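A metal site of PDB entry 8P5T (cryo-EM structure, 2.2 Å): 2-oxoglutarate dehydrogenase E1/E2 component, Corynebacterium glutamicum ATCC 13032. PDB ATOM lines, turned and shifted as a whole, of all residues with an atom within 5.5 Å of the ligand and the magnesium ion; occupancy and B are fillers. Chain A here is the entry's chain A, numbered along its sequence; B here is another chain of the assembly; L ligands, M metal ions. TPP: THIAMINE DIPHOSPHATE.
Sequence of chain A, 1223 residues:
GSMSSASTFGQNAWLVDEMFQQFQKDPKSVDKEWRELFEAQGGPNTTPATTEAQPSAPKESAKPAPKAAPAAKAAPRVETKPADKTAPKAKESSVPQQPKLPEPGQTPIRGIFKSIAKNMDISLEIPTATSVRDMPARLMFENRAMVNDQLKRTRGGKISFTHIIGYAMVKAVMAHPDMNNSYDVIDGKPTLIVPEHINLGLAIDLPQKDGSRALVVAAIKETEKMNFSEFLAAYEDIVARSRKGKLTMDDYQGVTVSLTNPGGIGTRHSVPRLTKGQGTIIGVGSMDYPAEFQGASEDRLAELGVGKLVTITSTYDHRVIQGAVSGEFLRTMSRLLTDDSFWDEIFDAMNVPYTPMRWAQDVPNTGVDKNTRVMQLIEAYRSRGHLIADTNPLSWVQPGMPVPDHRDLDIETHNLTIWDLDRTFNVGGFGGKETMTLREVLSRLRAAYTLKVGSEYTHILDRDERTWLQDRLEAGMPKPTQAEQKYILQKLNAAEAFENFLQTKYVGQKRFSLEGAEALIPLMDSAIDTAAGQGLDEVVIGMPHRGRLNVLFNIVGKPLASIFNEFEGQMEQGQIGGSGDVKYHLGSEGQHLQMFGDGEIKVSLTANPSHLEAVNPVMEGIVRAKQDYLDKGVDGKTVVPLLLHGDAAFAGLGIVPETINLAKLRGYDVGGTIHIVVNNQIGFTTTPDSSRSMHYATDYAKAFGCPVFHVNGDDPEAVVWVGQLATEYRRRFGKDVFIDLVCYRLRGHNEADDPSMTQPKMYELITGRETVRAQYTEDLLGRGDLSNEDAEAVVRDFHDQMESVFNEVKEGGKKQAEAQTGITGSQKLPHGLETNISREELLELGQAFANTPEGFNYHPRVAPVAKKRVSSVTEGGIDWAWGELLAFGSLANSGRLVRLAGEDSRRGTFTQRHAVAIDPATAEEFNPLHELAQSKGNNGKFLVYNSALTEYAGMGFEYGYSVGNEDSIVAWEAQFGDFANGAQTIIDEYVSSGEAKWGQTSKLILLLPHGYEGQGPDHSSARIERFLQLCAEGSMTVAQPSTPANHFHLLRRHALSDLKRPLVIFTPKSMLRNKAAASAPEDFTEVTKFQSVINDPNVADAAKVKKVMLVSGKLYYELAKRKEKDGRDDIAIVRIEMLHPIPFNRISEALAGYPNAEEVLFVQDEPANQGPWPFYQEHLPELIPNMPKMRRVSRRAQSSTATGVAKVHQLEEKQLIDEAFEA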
ATOM      1  N   HIS A 545      -8.141   3.381  -0.178  1.00  0.00           N
ATOM      2  CA  HIS A 545      -7.747   2.532  -1.298  1.00  0.00           C
ATOM      3  C   HIS A 545      -7.948   3.153  -2.676  1.00  0.00           C
ATOM      4  O   HIS A 545      -7.187   2.867  -3.587  1.00  0.00           O
ATOM      5  CB  HIS A 545      -8.560   1.232  -1.237  1.00  0.00           C
ATOM      6  CG  HIS A 545     -10.034   1.451  -1.190  1.00  0.00           C
ATOM      7  ND1 HIS A 545     -10.713   1.820  -0.043  1.00  0.00           N
ATOM      8  CD2 HIS A 545     -10.971   1.393  -2.148  1.00  0.00           C
ATOM      9  CE1 HIS A 545     -12.004   1.970  -0.317  1.00  0.00           C
ATOM     10  NE2 HIS A 545     -12.177   1.728  -1.589  1.00  0.00           N
ATOM     11  N   ARG A 546      -8.989   3.971  -2.842  1.00  0.00           N
ATOM     12  CA  ARG A 546      -9.435   4.441  -4.150  1.00  0.00           C
ATOM     13  C   ARG A 546      -8.426   5.403  -4.758  1.00  0.00           C
ATOM     14  O   ARG A 546      -8.364   6.575  -4.386  1.00  0.00           O
ATOM     15  CB  ARG A 546     -10.784   5.138  -3.967  1.00  0.00           C
ATOM     16  CG  ARG A 546     -11.442   5.730  -5.210  1.00  0.00           C
ATOM     17  CD  ARG A 546     -11.882   4.699  -6.209  1.00  0.00           C
ATOM     18  NE  ARG A 546     -12.869   3.782  -5.692  1.00  0.00           N
ATOM     19  CZ  ARG A 546     -13.059   2.555  -6.169  1.00  0.00           C
ATOM     20  NH1 ARG A 546     -12.375   2.127  -7.202  1.00  0.00           N
ATOM     21  NH2 ARG A 546     -13.911   1.751  -5.593  1.00  0.00           N
ATOM     22  N   SER A 610      -6.994  -1.574   6.550  1.00  0.00           N
ATOM     23  CA  SER A 610      -8.198  -1.629   5.752  1.00  0.00           C
ATOM     24  C   SER A 610      -9.371  -0.966   6.454  1.00  0.00           C
ATOM     25  O   SER A 610     -10.274  -0.468   5.797  1.00  0.00           O
ATOM     26  CB  SER A 610      -8.541  -3.041   5.417  1.00  0.00           C
ATOM     27  OG  SER A 610      -7.601  -3.576   4.487  1.00  0.00           O
ATOM     28  N   HIS A 611      -9.364  -0.956   7.790  1.00  0.00           N
ATOM     29  CA  HIS A 611     -10.394  -0.320   8.577  1.00  0.00           C
ATOM     30  C   HIS A 611     -10.484   1.148   8.196  1.00  0.00           C
ATOM     31  O   HIS A 611      -9.522   1.886   8.381  1.00  0.00           O
ATOM     32  CB  HIS A 611     -10.082  -0.436  10.057  1.00  0.00           C
ATOM     33  CG  HIS A 611     -10.092  -1.826  10.585  1.00  0.00           C
ATOM     34  ND1 HIS A 611      -9.272  -2.820  10.113  1.00  0.00           N
ATOM     35  CD2 HIS A 611     -10.784  -2.363  11.566  1.00  0.00           C
ATOM     36  CE1 HIS A 611      -9.521  -3.927  10.792  1.00  0.00           C
ATOM     37  NE2 HIS A 611     -10.429  -3.666  11.672  1.00  0.00           N
ATOM     38  N   LEU A 612     -11.637   1.570   7.689  1.00  0.00           N
ATOM     39  CA  LEU A 612     -11.797   2.902   7.133  1.00  0.00           C
ATOM     40  C   LEU A 612     -11.828   3.945   8.238  1.00  0.00           C
ATOM     41  O   LEU A 612     -12.432   3.722   9.279  1.00  0.00           O
ATOM     42  CB  LEU A 612     -13.099   2.925   6.326  1.00  0.00           C
ATOM     43  CG  LEU A 612     -13.075   2.139   5.011  1.00  0.00           C
ATOM     44  CD1 LEU A 612     -14.475   1.939   4.454  1.00  0.00           C
ATOM     45  CD2 LEU A 612     -12.227   2.835   3.973  1.00  0.00           C
ATOM     46  N   GLY A 646     -14.120   8.801   1.382  1.00  0.00           N
ATOM     47  CA  GLY A 646     -15.207   8.387   0.515  1.00  0.00           C
ATOM     48  C   GLY A 646     -16.554   8.748   1.107  1.00  0.00           C
ATOM     49  O   GLY A 646     -16.653   8.975   2.314  1.00  0.00           O
ATOM     50  N   ASP A 647     -17.607   8.770   0.287  1.00  0.00           N
ATOM     51  CA  ASP A 647     -18.880   9.363   0.656  1.00  0.00           C
ATOM     52  C   ASP A 647     -19.605   8.513   1.689  1.00  0.00           C
ATOM     53  O   ASP A 647     -20.099   9.053   2.680  1.00  0.00           O
ATOM     54  CB  ASP A 647     -19.744   9.661  -0.570  1.00  0.00           C
ATOM     55  CG  ASP A 647     -19.930   8.516  -1.545  1.00  0.00           C
ATOM     56  OD1 ASP A 647     -19.429   7.409  -1.263  1.00  0.00           O
ATOM     57  OD2 ASP A 647     -20.580   8.737  -2.599  1.00  0.00           O
ATOM     58  N   ALA A 648     -19.658   7.193   1.503  1.00  0.00           N
ATOM     59  CA  ALA A 648     -20.325   6.315   2.449  1.00  0.00           C
ATOM     60  C   ALA A 648     -19.626   6.312   3.796  1.00  0.00           C
ATOM     61  O   ALA A 648     -20.280   6.368   4.832  1.00  0.00           O
ATOM     62  CB  ALA A 648     -20.382   4.933   1.893  1.00  0.00           C
ATOM     63  N   ALA A 649     -18.295   6.278   3.802  1.00  0.00           N
ATOM     64  CA  ALA A 649     -17.543   6.211   5.035  1.00  0.00           C
ATOM     65  C   ALA A 649     -17.637   7.511   5.818  1.00  0.00           C
ATOM     66  O   ALA A 649     -17.672   7.483   7.047  1.00  0.00           O
ATOM     67  CB  ALA A 649     -16.122   5.889   4.728  1.00  0.00           C
ATOM     68  N   PHE A 650     -17.686   8.650   5.139  1.00  0.00           N
ATOM     69  CA  PHE A 650     -17.677   9.928   5.792  1.00  0.00           C
ATOM     70  C   PHE A 650     -18.966  10.162   6.566  1.00  0.00           C
ATOM     71  O   PHE A 650     -18.937  10.771   7.626  1.00  0.00           O
ATOM     72  CB  PHE A 650     -17.476  11.030   4.763  1.00  0.00           C
ATOM     73  CG  PHE A 650     -17.187  12.405   5.315  1.00  0.00           C
ATOM     74  CD1 PHE A 650     -15.906  12.803   5.590  1.00  0.00           C
ATOM     75  CD2 PHE A 650     -18.207  13.295   5.555  1.00  0.00           C
ATOM     76  CE1 PHE A 650     -15.649  14.068   6.083  1.00  0.00           C
ATOM     77  CE2 PHE A 650     -17.946  14.552   6.051  1.00  0.00           C
ATOM     78  CZ  PHE A 650     -16.671  14.941   6.309  1.00  0.00           C
ATOM     79  N   LEU A 653     -19.361   6.461   9.680  1.00  0.00           N
ATOM     80  CA  LEU A 653     -18.508   6.141  10.803  1.00  0.00           C
ATOM     81  C   LEU A 653     -18.388   7.340  11.723  1.00  0.00           C
ATOM     82  O   LEU A 653     -18.306   8.469  11.255  1.00  0.00           O
ATOM     83  CB  LEU A 653     -17.151   5.709  10.258  1.00  0.00           C
ATOM     84  CG  LEU A 653     -17.143   4.383   9.518  1.00  0.00           C
ATOM     85  CD1 LEU A 653     -15.840   4.191   8.776  1.00  0.00           C
ATOM     86  CD2 LEU A 653     -17.349   3.235  10.467  1.00  0.00           C
ATOM     87  N   VAL A 678     -14.550  12.258  -2.092  1.00  0.00           N
ATOM     88  CA  VAL A 678     -14.729  11.749  -3.441  1.00  0.00           C
ATOM     89  C   VAL A 678     -16.108  11.125  -3.535  1.00  0.00           C
ATOM     90  O   VAL A 678     -16.296   9.987  -3.169  1.00  0.00           O
ATOM     91  CB  VAL A 678     -13.625  10.763  -3.823  1.00  0.00           C
ATOM     92  CG1 VAL A 678     -13.731  10.306  -5.250  1.00  0.00           C
ATOM     93  CG2 VAL A 678     -12.255  11.326  -3.598  1.00  0.00           C
ATOM     94  N   ASN A 679     -17.065  11.885  -4.055  1.00  0.00           N
ATOM     95  CA  ASN A 679     -18.469  11.543  -4.057  1.00  0.00           C
ATOM     96  C   ASN A 679     -18.808  10.923  -5.399  1.00  0.00           C
ATOM     97  O   ASN A 679     -19.104  11.636  -6.355  1.00  0.00           O
ATOM     98  CB  ASN A 679     -19.275  12.795  -3.755  1.00  0.00           C
ATOM     99  CG  ASN A 679     -20.755  12.553  -3.620  1.00  0.00           C
ATOM    100  OD1 ASN A 679     -21.178  11.623  -2.931  1.00  0.00           O
ATOM    101  ND2 ASN A 679     -21.554  13.372  -4.273  1.00  0.00           N
ATOM    102  N   ASN A 680     -18.755   9.592  -5.473  1.00  0.00           N
ATOM    103  CA  ASN A 680     -19.017   8.866  -6.699  1.00  0.00           C
ATOM    104  C   ASN A 680     -20.350   8.142  -6.623  1.00  0.00           C
ATOM    105  O   ASN A 680     -20.621   7.250  -7.410  1.00  0.00           O
ATOM    106  CB  ASN A 680     -17.868   7.933  -7.030  1.00  0.00           C
ATOM    107  CG  ASN A 680     -17.599   6.883  -5.999  1.00  0.00           C
ATOM    108  OD1 ASN A 680     -18.413   6.659  -5.124  1.00  0.00           O
ATOM    109  ND2 ASN A 680     -16.465   6.214  -6.113  1.00  0.00           N
ATOM    110  N   GLN A 681     -21.171   8.543  -5.671  1.00  0.00           N
ATOM    111  CA  GLN A 681     -22.593   8.260  -5.652  1.00  0.00           C
ATOM    112  C   GLN A 681     -22.864   6.786  -5.442  1.00  0.00           C
ATOM    113  O   GLN A 681     -23.895   6.297  -5.871  1.00  0.00           O
ATOM    114  CB  GLN A 681     -23.209   8.827  -6.920  1.00  0.00           C
ATOM    115  CG  GLN A 681     -22.885  10.295  -7.120  1.00  0.00           C
ATOM    116  CD  GLN A 681     -23.550  10.883  -8.335  1.00  0.00           C
ATOM    117  OE1 GLN A 681     -24.762  11.059  -8.365  1.00  0.00           O
ATOM    118  NE2 GLN A 681     -22.757  11.188  -9.342  1.00  0.00           N
ATOM    119  N   ILE A 682     -21.978   6.076  -4.735  1.00  0.00           N
ATOM    120  CA  ILE A 682     -22.152   4.657  -4.506  1.00  0.00           C
ATOM    121  C   ILE A 682     -21.161   4.161  -3.464  1.00  0.00           C
ATOM    122  O   ILE A 682     -20.044   4.628  -3.385  1.00  0.00           O
ATOM    123  CB  ILE A 682     -22.045   3.883  -5.831  1.00  0.00           C
ATOM    124  CG1 ILE A 682     -22.510   2.439  -5.667  1.00  0.00           C
ATOM    125  CG2 ILE A 682     -20.652   3.953  -6.402  1.00  0.00           C
ATOM    126  CD1 ILE A 682     -23.124   1.866  -6.906  1.00  0.00           C
ATOM    127  N   GLY A 683     -21.613   3.171  -2.684  1.00  0.00           N
ATOM    128  CA  GLY A 683     -20.826   2.510  -1.662  1.00  0.00           C
ATOM    129  C   GLY A 683     -20.074   1.324  -2.242  1.00  0.00           C
ATOM    130  O   GLY A 683     -19.044   1.517  -2.889  1.00  0.00           O
ATOM    131  N   PHE A 684     -20.569   0.119  -1.997  1.00  0.00           N
ATOM    132  CA  PHE A 684     -20.084  -1.064  -2.692  1.00  0.00           C
ATOM    133  C   PHE A 684     -21.232  -1.517  -3.588  1.00  0.00           C
ATOM    134  O   PHE A 684     -21.125  -1.453  -4.814  1.00  0.00           O
ATOM    135  CB  PHE A 684     -19.580  -2.065  -1.648  1.00  0.00           C
ATOM    136  CG  PHE A 684     -19.188  -3.439  -2.111  1.00  0.00           C
ATOM    137  CD1 PHE A 684     -19.330  -3.860  -3.427  1.00  0.00           C
ATOM    138  CD2 PHE A 684     -18.675  -4.348  -1.204  1.00  0.00           C
ATOM    139  CE1 PHE A 684     -18.973  -5.139  -3.811  1.00  0.00           C
ATOM    140  CE2 PHE A 684     -18.316  -5.623  -1.580  1.00  0.00           C
ATOM    141  CZ  PHE A 684     -18.460  -6.017  -2.885  1.00  0.00           C
ATOM    142  N   ARG A 745     -18.086   6.163 -10.698  1.00  0.00           N
ATOM    143  CA  ARG A 745     -17.218   4.987 -10.693  1.00  0.00           C
ATOM    144  C   ARG A 745     -17.480   4.167 -11.952  1.00  0.00           C
ATOM    145  O   ARG A 745     -18.576   3.656 -12.109  1.00  0.00           O
ATOM    146  CB  ARG A 745     -17.534   4.170  -9.448  1.00  0.00           C
ATOM    147  CG  ARG A 745     -16.547   3.074  -9.112  1.00  0.00           C
ATOM    148  CD  ARG A 745     -17.060   2.136  -8.055  1.00  0.00           C
ATOM    149  NE  ARG A 745     -18.165   1.335  -8.561  1.00  0.00           N
ATOM    150  CZ  ARG A 745     -19.012   0.660  -7.808  1.00  0.00           C
ATOM    151  NH1 ARG A 745     -18.866   0.606  -6.507  1.00  0.00           N
ATOM    152  NH2 ARG A 745     -20.020   0.027  -8.368  1.00  0.00           N
ATOM    153  N   HIS A 749     -16.826  -2.290  -7.874  1.00  0.00           N
ATOM    154  CA  HIS A 749     -16.119  -1.932  -6.668  1.00  0.00           C
ATOM    155  C   HIS A 749     -14.662  -2.335  -6.835  1.00  0.00           C
ATOM    156  O   HIS A 749     -13.763  -1.555  -6.521  1.00  0.00           O
ATOM    157  CB  HIS A 749     -16.745  -2.602  -5.446  1.00  0.00           C
ATOM    158  CG  HIS A 749     -16.130  -2.154  -4.164  1.00  0.00           C
ATOM    159  ND1 HIS A 749     -15.333  -2.965  -3.395  1.00  0.00           N
ATOM    160  CD2 HIS A 749     -16.150  -0.981  -3.562  1.00  0.00           C
ATOM    161  CE1 HIS A 749     -14.919  -2.282  -2.351  1.00  0.00           C
ATOM    162  NE2 HIS A 749     -15.402  -1.073  -2.421  1.00  0.00           N
ATOM    163  N   GLU B 903     -23.997  -5.184   6.059  1.00  0.00           N
ATOM    164  CA  GLU B 903     -23.478  -4.468   4.907  1.00  0.00           C
ATOM    165  C   GLU B 903     -23.529  -5.344   3.667  1.00  0.00           C
ATOM    166  O   GLU B 903     -22.854  -6.368   3.607  1.00  0.00           O
ATOM    167  CB  GLU B 903     -22.034  -4.028   5.116  1.00  0.00           C
ATOM    168  CG  GLU B 903     -21.873  -2.870   6.093  1.00  0.00           C
ATOM    169  CD  GLU B 903     -20.443  -2.584   6.532  1.00  0.00           C
ATOM    170  OE1 GLU B 903     -20.266  -1.810   7.500  1.00  0.00           O
ATOM    171  OE2 GLU B 903     -19.510  -3.137   5.900  1.00  0.00           O
ATOM    172  N   LEU B 949     -22.769   2.122   6.909  1.00  0.00           N
ATOM    173  CA  LEU B 949     -21.419   1.653   7.136  1.00  0.00           C
ATOM    174  C   LEU B 949     -21.027   1.930   8.589  1.00  0.00           C
ATOM    175  O   LEU B 949     -20.332   2.897   8.881  1.00  0.00           O
ATOM    176  CB  LEU B 949     -20.501   2.359   6.128  1.00  0.00           C
ATOM    177  CG  LEU B 949     -19.282   1.566   5.672  1.00  0.00           C
ATOM    178  CD1 LEU B 949     -18.614   2.252   4.499  1.00  0.00           C
ATOM    179  CD2 LEU B 949     -18.277   1.404   6.800  1.00  0.00           C
ATOM    180  N   GLU B 951     -20.378  -0.466  12.500  1.00  0.00           N
ATOM    181  CA  GLU B 951     -20.346  -1.732  13.207  1.00  0.00           C
ATOM    182  C   GLU B 951     -20.863  -1.568  14.626  1.00  0.00           C
ATOM    183  O   GLU B 951     -21.479  -2.482  15.169  1.00  0.00           O
ATOM    184  CB  GLU B 951     -18.926  -2.311  13.209  1.00  0.00           C
ATOM    185  CG  GLU B 951     -18.534  -2.964  11.899  1.00  0.00           C
ATOM    186  CD  GLU B 951     -18.007  -2.057  10.806  1.00  0.00           C
ATOM    187  OE1 GLU B 951     -17.902  -0.834  11.040  1.00  0.00           O
ATOM    188  OE2 GLU B 951     -17.697  -2.586   9.706  1.00  0.00           O
ATOM    189  N   GLN B 975     -19.165  -7.808   7.081  1.00  0.00           N
ATOM    190  CA  GLN B 975     -18.634  -7.937   5.734  1.00  0.00           C
ATOM    191  C   GLN B 975     -17.449  -8.873   5.749  1.00  0.00           C
ATOM    192  O   GLN B 975     -17.372  -9.788   4.951  1.00  0.00           O
ATOM    193  CB  GLN B 975     -18.302  -6.556   5.174  1.00  0.00           C
ATOM    194  CG  GLN B 975     -17.819  -6.608   3.753  1.00  0.00           C
ATOM    195  CD  GLN B 975     -18.228  -5.395   2.954  1.00  0.00           C
ATOM    196  OE1 GLN B 975     -17.397  -4.597   2.543  1.00  0.00           O
ATOM    197  NE2 GLN B 975     -19.515  -5.287   2.689  1.00  0.00           N
ATOM    198  N   PHE B 979     -13.717  -6.857  11.039  1.00  0.00           N
ATOM    199  CA  PHE B 979     -14.195  -5.515  11.311  1.00  0.00           C
ATOM    200  C   PHE B 979     -15.105  -5.489  12.534  1.00  0.00           C
ATOM    201  O   PHE B 979     -15.656  -4.447  12.852  1.00  0.00           O
ATOM    202  CB  PHE B 979     -14.891  -4.975  10.074  1.00  0.00           C
ATOM    203  CG  PHE B 979     -14.010  -4.848   8.860  1.00  0.00           C
ATOM    204  CD1 PHE B 979     -12.798  -4.209   8.931  1.00  0.00           C
ATOM    205  CD2 PHE B 979     -14.404  -5.373   7.651  1.00  0.00           C
ATOM    206  CE1 PHE B 979     -11.974  -4.105   7.820  1.00  0.00           C
ATOM    207  CE2 PHE B 979     -13.582  -5.273   6.532  1.00  0.00           C
ATOM    208  CZ  PHE B 979     -12.374  -4.647   6.635  1.00  0.00           C
HETATM  209  N1' TPP L   1     -16.069  -1.256   7.710  1.00  0.00           N
HETATM  210  C2' TPP L   1     -14.834  -0.806   7.900  1.00  0.00           C
HETATM  211  CM2 TPP L   1     -14.550  -0.113   9.197  1.00  0.00           C
HETATM  212  N3' TPP L   1     -13.827  -0.942   7.038  1.00  0.00           N
HETATM  213  C4' TPP L   1     -14.082  -1.566   5.884  1.00  0.00           C
HETATM  214  N4' TPP L   1     -13.045  -1.692   5.041  1.00  0.00           N
HETATM  215  C5' TPP L   1     -15.359  -2.067   5.581  1.00  0.00           C
HETATM  216  C6' TPP L   1     -16.316  -1.878   6.552  1.00  0.00           C
HETATM  217  C7' TPP L   1     -15.687  -2.771   4.282  1.00  0.00           C
HETATM  218  N3  TPP L   1     -15.700  -1.886   3.111  1.00  0.00           N
HETATM  219  C2  TPP L   1     -14.658  -1.764   2.262  1.00  0.00           C
HETATM  220  S1  TPP L   1     -15.023  -0.675   1.087  1.00  0.00           S
HETATM  221  C5  TPP L   1     -16.529  -0.335   1.579  1.00  0.00           C
HETATM  222  C4  TPP L   1     -16.782  -1.081   2.716  1.00  0.00           C
HETATM  223  CM4 TPP L   1     -18.056  -1.053   3.514  1.00  0.00           C
HETATM  224  C6  TPP L   1     -17.306   0.641   0.785  1.00  0.00           C
HETATM  225  C7  TPP L   1     -16.768   2.014   0.956  1.00  0.00           C
HETATM  226  O7  TPP L   1     -17.598   2.947   0.239  1.00  0.00           O
HETATM  227  PA  TPP L   1     -17.049   4.409  -0.047  1.00  0.00           P
HETATM  228  O1A TPP L   1     -18.045   5.139  -0.870  1.00  0.00           O
HETATM  229  O2A TPP L   1     -16.605   5.016   1.219  1.00  0.00           O
HETATM  230  O3A TPP L   1     -15.804   4.076  -0.990  1.00  0.00           O
HETATM  231  PB  TPP L   1     -15.565   4.034  -2.570  1.00  0.00           P
HETATM  232  O1B TPP L   1     -15.562   2.614  -2.935  1.00  0.00           O
HETATM  233  O2B TPP L   1     -16.713   4.775  -3.110  1.00  0.00           O
HETATM  234  O3B TPP L   1     -14.276   4.699  -2.837  1.00  0.00           O
HETATM  235 MG    MG M   1     -18.361   6.113  -2.962  1.00  0.00          MG
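The magnesium ion is bound by an oxygen (O2B) of the ligand (2.1 Å), the side-chain amide oxygen (OD1) of Asn 680 (2.2 Å), the backbone carbonyl oxygen (O) of Ile 682 (2.3 Å), an oxygen (O1A) of the ligand (2.3 Å) and the side-chain carboxylate (OD1) of Asp 647 (2.4 Å). The magnesium ion has five donor atoms within binding distance.
The side-chain carboxylate (OE2) of Glu 951 of chain B is in hydrogen-bond range of a nitrogen (N1') of the ligand. N of Leu 612 sits at hydrogen-bond distance from N3' of the ligand. O1B of the ligand lies within salt-bridge range of NH2 of Arg 546 (3.2 Å). A ring nitrogen (NE2) of His 749 lies close to a sulfur (S1) of the ligand (3.6 Å). The backbone NH of Ala 649 lies within hydrogen-bond range of an oxygen (O2A) of the ligand, 3.3 Å away. A nitrogen (N4') of the ligand is in hydrogen-bond range of the backbone carbonyl oxygen (O) of Ser 610, at 3.1 Å.
A nitrogen (N3) of the ligand lies close to the side-chain amide oxygen of Gln 975 of chain B, 3.2 Å away. NE2 of His 545 touches O1B of the ligand, 3.7 Å away. His 611 touches the ligand. CA of Gly 646 touches O2A of the ligand, at 3.7 Å. Ala 648 touches the ligand (N to O1A, 3.5 Å). O of Gly 683 touches O1B of the ligand (3.7 Å). OE2 of Glu 903 of chain B touches CM4 of the ligand (3.5 Å). Leu 949 of chain B touches the ligand. Phe 979 of chain B touches the ligand (CZ to N4', 3.4 Å). 18 residues have an atom within 4 Å of the ligand: His 545, Arg 546, Ser 610, His 611, Leu 612, Gly 646, Asp 647, Ala 648, Ala 649, Asn 680, Ile 682, Gly 683, His 749, Glu 903 of chain B, Leu 949 of chain B, Glu 951 of chain B, Gln 975 of chain B and Phe 979 of chain B. The nearest printed residue that does not touch the ligand is Phe 684 (4.3 Å).
The side-chain carboxylate of Asp 647 sits at hydrogen-bond distance from the backbone NH of Gln 681 (3.1 Å). The guanidinium group (NH2) of Arg 546 is in hydrogen-bond range of the backbone carbonyl oxygen (O) of His 749. OD2 of Asp 647 sits close to OD1 of Asn 679, 3.0 Å away.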
